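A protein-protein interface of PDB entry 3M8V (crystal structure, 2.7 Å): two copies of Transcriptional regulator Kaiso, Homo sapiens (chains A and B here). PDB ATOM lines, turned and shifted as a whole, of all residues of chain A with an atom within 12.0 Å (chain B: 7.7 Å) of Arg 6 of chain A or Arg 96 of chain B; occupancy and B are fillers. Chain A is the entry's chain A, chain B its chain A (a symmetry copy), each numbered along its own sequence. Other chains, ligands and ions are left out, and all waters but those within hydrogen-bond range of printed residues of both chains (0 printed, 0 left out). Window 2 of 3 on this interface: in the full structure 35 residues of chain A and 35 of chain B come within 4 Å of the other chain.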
ATOM      1  N   ARG A   6     -14.374 -33.749  28.258  1.00  0.00           N
ATOM      2  CA  ARG A   6     -14.597 -32.316  28.484  1.00  0.00           C
ATOM      3  C   ARG A   6     -13.777 -31.420  27.519  1.00  0.00           C
ATOM      4  O   ARG A   6     -12.592 -31.147  27.751  1.00  0.00           O
ATOM      5  CB  ARG A   6     -14.310 -31.976  29.957  1.00  0.00           C
ATOM      6  CG  ARG A   6     -14.755 -30.595  30.440  1.00  0.00           C
ATOM      7  CD  ARG A   6     -16.254 -30.447  30.374  1.00  0.00           C
ATOM      8  NE  ARG A   6     -16.721 -30.536  28.994  1.00  0.00           N
ATOM      9  CZ  ARG A   6     -17.825 -31.175  28.612  1.00  0.00           C
ATOM     10  NH1 ARG A   6     -18.592 -31.785  29.514  1.00  0.00           N
ATOM     11  NH2 ARG A   6     -18.166 -31.202  27.325  1.00  0.00           N
ATOM     12  N   LYS A   7     -14.413 -30.976  26.434  1.00  0.00           N
ATOM     13  CA  LYS A   7     -13.729 -30.185  25.424  1.00  0.00           C
ATOM     14  C   LYS A   7     -14.661 -29.281  24.626  1.00  0.00           C
ATOM     15  O   LYS A   7     -15.847 -29.570  24.496  1.00  0.00           O
ATOM     16  CB  LYS A   7     -12.967 -31.102  24.463  1.00  0.00           C
ATOM     17  CG  LYS A   7     -13.819 -31.793  23.406  1.00  0.00           C
ATOM     18  CD  LYS A   7     -12.979 -32.712  22.510  1.00  0.00           C
ATOM     19  CE  LYS A   7     -13.787 -33.936  22.050  1.00  0.00           C
ATOM     20  NZ  LYS A   7     -12.956 -35.106  21.643  1.00  0.00           N
ATOM     21  N   LEU A   8     -14.116 -28.197  24.075  1.00  0.00           N
ATOM     22  CA  LEU A   8     -14.893 -27.315  23.206  1.00  0.00           C
ATOM     23  C   LEU A   8     -14.476 -27.418  21.749  1.00  0.00           C
ATOM     24  O   LEU A   8     -13.293 -27.402  21.417  1.00  0.00           O
ATOM     25  CB  LEU A   8     -14.770 -25.864  23.650  1.00  0.00           C
ATOM     26  CG  LEU A   8     -15.058 -25.600  25.132  1.00  0.00           C
ATOM     27  CD1 LEU A   8     -14.773 -24.151  25.457  1.00  0.00           C
ATOM     28  CD2 LEU A   8     -16.491 -25.982  25.535  1.00  0.00           C
ATOM     29  N   ILE A   9     -15.471 -27.500  20.879  1.00  0.00           N
ATOM     30  CA  ILE A   9     -15.235 -27.606  19.455  1.00  0.00           C
ATOM     31  C   ILE A   9     -15.673 -26.359  18.711  1.00  0.00           C
ATOM     32  O   ILE A   9     -16.757 -25.840  18.939  1.00  0.00           O
ATOM     33  CB  ILE A   9     -15.998 -28.793  18.889  1.00  0.00           C
ATOM     34  CG1 ILE A   9     -15.582 -30.048  19.631  1.00  0.00           C
ATOM     35  CG2 ILE A   9     -15.672 -28.971  17.429  1.00  0.00           C
ATOM     36  CD1 ILE A   9     -14.080 -30.244  19.570  1.00  0.00           C
ATOM     37  N   SER A  10     -14.824 -25.871  17.820  1.00  0.00           N
ATOM     38  CA  SER A  10     -15.211 -24.789  16.919  1.00  0.00           C
ATOM     39  C   SER A  10     -14.947 -25.264  15.514  1.00  0.00           C
ATOM     40  O   SER A  10     -13.959 -25.949  15.260  1.00  0.00           O
ATOM     41  CB  SER A  10     -14.413 -23.515  17.187  1.00  0.00           C
ATOM     42  OG  SER A  10     -14.543 -23.118  18.538  1.00  0.00           O
ATOM     43  N   ALA A  11     -15.846 -24.920  14.602  1.00  0.00           N
ATOM     44  CA  ALA A  11     -15.635 -25.225  13.203  1.00  0.00           C
ATOM     45  C   ALA A  11     -16.002 -24.015  12.369  1.00  0.00           C
ATOM     46  O   ALA A  11     -16.953 -23.300  12.683  1.00  0.00           O
ATOM     47  CB  ALA A  11     -16.457 -26.426  12.788  1.00  0.00           C
ATOM     48  N   ARG B  76     -33.959 -29.385  20.363  1.00  0.00           N
ATOM     49  CA  ARG B  76     -33.991 -28.474  21.504  1.00  0.00           C
ATOM     50  C   ARG B  76     -33.676 -27.042  21.083  1.00  0.00           C
ATOM     51  O   ARG B  76     -32.929 -26.805  20.137  1.00  0.00           O
ATOM     52  CB  ARG B  76     -33.017 -28.920  22.595  1.00  0.00           C
ATOM     53  CG  ARG B  76     -33.280 -30.311  23.137  1.00  0.00           C
ATOM     54  CD  ARG B  76     -32.633 -30.529  24.502  1.00  0.00           C
ATOM     55  NE  ARG B  76     -31.176 -30.579  24.437  1.00  0.00           N
ATOM     56  CZ  ARG B  76     -30.368 -29.685  25.000  1.00  0.00           C
ATOM     57  NH1 ARG B  76     -30.874 -28.659  25.682  1.00  0.00           N
ATOM     58  NH2 ARG B  76     -29.052 -29.821  24.885  1.00  0.00           N
ATOM     59  N   GLU B  78     -31.790 -24.634  22.416  1.00  0.00           N
ATOM     60  CA  GLU B  78     -30.391 -24.197  22.447  1.00  0.00           C
ATOM     61  C   GLU B  78     -29.596 -24.783  21.290  1.00  0.00           C
ATOM     62  O   GLU B  78     -28.654 -24.168  20.800  1.00  0.00           O
ATOM     63  CB  GLU B  78     -29.717 -24.499  23.791  1.00  0.00           C
ATOM     64  CG  GLU B  78     -29.347 -25.965  24.030  1.00  0.00           C
ATOM     65  CD  GLU B  78     -28.401 -26.154  25.226  1.00  0.00           C
ATOM     66  OE1 GLU B  78     -27.511 -25.294  25.421  1.00  0.00           O
ATOM     67  OE2 GLU B  78     -28.550 -27.160  25.968  1.00  0.00           O
ATOM     68  N   GLU B  82     -27.871 -22.677  17.907  1.00  0.00           N
ATOM     69  CA  GLU B  82     -26.558 -22.926  17.302  1.00  0.00           C
ATOM     70  C   GLU B  82     -26.619 -23.038  15.772  1.00  0.00           C
ATOM     71  O   GLU B  82     -25.786 -22.476  15.062  1.00  0.00           O
ATOM     72  CB  GLU B  82     -25.938 -24.205  17.879  1.00  0.00           C
ATOM     73  CG  GLU B  82     -24.616 -24.028  18.622  1.00  0.00           C
ATOM     74  CD  GLU B  82     -23.957 -22.682  18.366  1.00  0.00           C
ATOM     75  OE1 GLU B  82     -24.470 -21.677  18.897  1.00  0.00           O
ATOM     76  OE2 GLU B  82     -22.926 -22.629  17.653  1.00  0.00           O
ATOM     77  N   VAL B  93     -18.995 -22.060  17.422  1.00  0.00           N
ATOM     78  CA  VAL B  93     -17.908 -21.534  18.221  1.00  0.00           C
ATOM     79  C   VAL B  93     -17.961 -22.097  19.628  1.00  0.00           C
ATOM     80  O   VAL B  93     -18.943 -21.907  20.349  1.00  0.00           O
ATOM     81  CB  VAL B  93     -17.964 -19.996  18.271  1.00  0.00           C
ATOM     82  CG1 VAL B  93     -16.773 -19.428  19.060  1.00  0.00           C
ATOM     83  CG2 VAL B  93     -17.991 -19.425  16.866  1.00  0.00           C
ATOM     84  N   ARG B  94     -16.900 -22.804  20.007  1.00  0.00           N
ATOM     85  CA  ARG B  94     -16.780 -23.363  21.348  1.00  0.00           C
ATOM     86  C   ARG B  94     -18.018 -24.101  21.819  1.00  0.00           C
ATOM     87  O   ARG B  94     -18.478 -23.925  22.938  1.00  0.00           O
ATOM     88  CB  ARG B  94     -16.425 -22.279  22.364  1.00  0.00           C
ATOM     89  CG  ARG B  94     -14.998 -21.771  22.286  1.00  0.00           C
ATOM     90  CD  ARG B  94     -14.671 -20.930  23.514  1.00  0.00           C
ATOM     91  NE  ARG B  94     -15.505 -19.729  23.584  1.00  0.00           N
ATOM     92  CZ  ARG B  94     -16.497 -19.522  24.459  1.00  0.00           C
ATOM     93  NH1 ARG B  94     -17.188 -18.385  24.410  1.00  0.00           N
ATOM     94  NH2 ARG B  94     -16.806 -20.434  25.381  1.00  0.00           N
ATOM     95  N   VAL B  95     -18.548 -24.929  20.942  1.00  0.00           N
ATOM     96  CA  VAL B  95     -19.600 -25.868  21.288  1.00  0.00           C
ATOM     97  C   VAL B  95     -19.049 -26.985  22.170  1.00  0.00           C
ATOM     98  O   VAL B  95     -17.977 -27.516  21.896  1.00  0.00           O
ATOM     99  CB  VAL B  95     -20.155 -26.488  20.000  1.00  0.00           C
ATOM    100  CG1 VAL B  95     -21.230 -27.496  20.302  1.00  0.00           C
ATOM    101  CG2 VAL B  95     -20.667 -25.406  19.098  1.00  0.00           C
ATOM    102  N   ARG B  96     -19.775 -27.356  23.222  1.00  0.00           N
ATOM    103  CA  ARG B  96     -19.290 -28.419  24.103  1.00  0.00           C
ATOM    104  C   ARG B  96     -19.464 -29.825  23.505  1.00  0.00           C
ATOM    105  O   ARG B  96     -20.479 -30.131  22.889  1.00  0.00           O
ATOM    106  CB  ARG B  96     -19.808 -28.280  25.555  1.00  0.00           C
ATOM    107  CG  ARG B  96     -21.306 -28.253  25.765  1.00  0.00           C
ATOM    108  CD  ARG B  96     -21.677 -27.898  27.222  1.00  0.00           C
ATOM    109  NE  ARG B  96     -21.317 -28.934  28.196  1.00  0.00           N
ATOM    110  CZ  ARG B  96     -22.170 -29.813  28.724  1.00  0.00           C
ATOM    111  NH1 ARG B  96     -23.454 -29.793  28.379  1.00  0.00           N
ATOM    112  NH2 ARG B  96     -21.744 -30.712  29.605  1.00  0.00           N
ATOM    113  N   SER B  97     -18.443 -30.660  23.680  1.00  0.00           N
ATOM    114  CA  SER B  97     -18.289 -31.900  22.918  1.00  0.00           C
ATOM    115  C   SER B  97     -19.460 -32.881  22.968  1.00  0.00           C
ATOM    116  O   SER B  97     -19.641 -33.670  22.049  1.00  0.00           O
ATOM    117  CB  SER B  97     -16.996 -32.617  23.325  1.00  0.00           C
ATOM    118  OG  SER B  97     -16.964 -32.887  24.723  1.00  0.00           O
ATOM    119  N   ASP B  98     -20.249 -32.860  24.032  1.00  0.00           N
ATOM    120  CA  ASP B  98     -21.354 -33.812  24.117  1.00  0.00           C
ATOM    121  C   ASP B  98     -22.583 -33.367  23.306  1.00  0.00           C
ATOM    122  O   ASP B  98     -23.293 -34.199  22.733  1.00  0.00           O
ATOM    123  CB  ASP B  98     -21.698 -34.133  25.577  1.00  0.00           C
ATOM    124  CG  ASP B  98     -21.886 -32.893  26.422  1.00  0.00           C
ATOM    125  OD1 ASP B  98     -22.600 -31.972  25.980  1.00  0.00           O
ATOM    126  OD2 ASP B  98     -21.321 -32.838  27.532  1.00  0.00           O
ATOM    127  N   LEU B  99     -22.806 -32.055  23.239  1.00  0.00           N
ATOM    128  CA  LEU B  99     -23.905 -31.491  22.458  1.00  0.00           C
ATOM    129  C   LEU B  99     -23.698 -31.700  20.970  1.00  0.00           C
ATOM    130  O   LEU B  99     -24.591 -31.464  20.161  1.00  0.00           O
ATOM    131  CB  LEU B  99     -24.050 -29.995  22.729  1.00  0.00           C
ATOM    132  CG  LEU B  99     -24.485 -29.590  24.135  1.00  0.00           C
ATOM    133  CD1 LEU B  99     -24.806 -28.109  24.149  1.00  0.00           C
ATOM    134  CD2 LEU B  99     -25.693 -30.410  24.596  1.00  0.00           C
ATOM    135  N   LEU B 100     -22.510 -32.157  20.615  1.00  0.00           N
ATOM    136  CA  LEU B 100     -22.137 -32.250  19.218  1.00  0.00           C
ATOM    137  C   LEU B 100     -22.977 -33.264  18.474  1.00  0.00           C
ATOM    138  O   LEU B 100     -23.521 -32.984  17.406  1.00  0.00           O
ATOM    139  CB  LEU B 100     -20.657 -32.611  19.087  1.00  0.00           C
ATOM    140  CG  LEU B 100     -20.022 -32.099  17.797  1.00  0.00           C
ATOM    141  CD1 LEU B 100     -20.031 -30.569  17.772  1.00  0.00           C
ATOM    142  CD2 LEU B 100     -18.611 -32.655  17.635  1.00  0.00           C
ATOM    143  N   ASP B 101     -23.076 -34.452  19.041  1.00  0.00           N
ATOM    144  CA  ASP B 101     -23.782 -35.524  18.378  1.00  0.00           C
ATOM    145  C   ASP B 101     -25.198 -35.069  18.091  1.00  0.00           C
ATOM    146  O   ASP B 101     -25.759 -35.360  17.036  1.00  0.00           O
ATOM    147  CB  ASP B 101     -23.775 -36.769  19.249  1.00  0.00           C
ATOM    148  CG  ASP B 101     -23.466 -38.009  18.456  1.00  0.00           C
ATOM    149  OD1 ASP B 101     -24.399 -38.803  18.205  1.00  0.00           O
ATOM    150  OD2 ASP B 101     -22.293 -38.171  18.061  1.00  0.00           O
ATOM    151  N   LEU B 103     -26.206 -31.841  17.874  1.00  0.00           N
ATOM    152  CA  LEU B 103     -26.110 -30.774  16.883  1.00  0.00           C
ATOM    153  C   LEU B 103     -26.040 -31.367  15.472  1.00  0.00           C
ATOM    154  O   LEU B 103     -26.754 -30.930  14.565  1.00  0.00           O
ATOM    155  CB  LEU B 103     -24.873 -29.905  17.167  1.00  0.00           C
ATOM    156  CG  LEU B 103     -24.542 -28.724  16.243  1.00  0.00           C
ATOM    157  CD1 LEU B 103     -25.684 -27.718  16.184  1.00  0.00           C
ATOM    158  CD2 LEU B 103     -23.255 -28.026  16.676  1.00  0.00           C
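Of the 6 printed residues of chain A, 5 touch a printed residue of chain B.
Hydrophobic or aromatic side chains of chain A that line the printed part of chain B: Leu 8 and Ile 9.
Of the 13 printed residues of chain B, 6 touch a printed residue of chain A.
The backbone carbonyl oxygen (O) of Ile 9 of chain A sits at hydrogen-bond distance from the backbone NH (N) of Arg 94 of chain B (3.2 Å).
The guanidinium group (NH1) of Arg 6 of chain A lies within salt-bridge range of the side-chain carboxylate (OD2) of Asp 98 of chain B (3.5 Å).
OG of Ser 97 of chain B is in hydrogen-bond range of NH2 of Arg 6 of chain A (3.3 Å).
NH2 of Arg 96 of chain B lies close to NH1 of Arg 6 of chain A, 3.3 Å away.
The backbone NH of Arg 94 of chain B lies within hydrogen-bond range of the side-chain hydroxyl of Ser 10 of chain A (2.8 Å).
The backbone carbonyl oxygen (O) of Val 95 of chain B is in hydrogen-bond range of the backbone NH (N) of Ile 9 of chain A (2.7 Å).
O of Lys 7 of chain A lies within hydrogen-bond range of N of Ser 97 of chain B (2.9 Å).
No position is printed for both chains.
The side-chain carboxylate (OD2) of Asp 98 of chain B lies within salt-bridge range of the guanidinium group (NH2) of Arg 96 of chain B, 3.0 Å away.
Among the printed residues, merely in contact across the chains: Leu 8 of chain A with Val 95 of chain B (3.4 Å), Lys 7 of chain A with Arg 96 of chain B (3.7 Å), Ser 10 of chain A with Val 93 of chain B (3.7 Å), Leu 8 of chain A with Arg 94 of chain B (3.8 Å), Lys 7 of chain A with Val 95 of chain B (3.9 Å), Leu 8 of chain A with Arg 96 of chain B (3.98 Å) and Ile 9 of chain A with Val 93 of chain B (3.99 Å).
Of chain B, only Arg 96, Ser 97 and Asp 98 come within 4 Å of Arg 6 of chain A.
Of the printed residues of chain B, Lys 7 of chain A touches Val 95 (3.9 Å), Arg 96 (3.7 Å) and Ser 97 (2.9 Å).
Of the printed residues of chain B, Ile 9 of chain A touches Val 93, Arg 94 and Val 95.
Of the printed residues of chain B, Ser 10 of chain A touches Val 93 (3.7 Å) and Arg 94 (2.8 Å).
Of the printed residues of chain A, Val 93 of chain B touches Ile 9 (3.99 Å) and Ser 10 (3.7 Å).
Printed residues of chain A within 4 Å of Arg 94 of chain B: Leu 8, Ile 9 and Ser 10.
Of the printed residues of chain A, Ser 97 of chain B touches Arg 6 (3.3 Å) and Lys 7 (2.9 Å).
Of chain A, only Arg 6 comes within 4 Å of Asp 98 of chain B.
No residue of chain A comes within 4 Å of Leu 100 of chain B.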
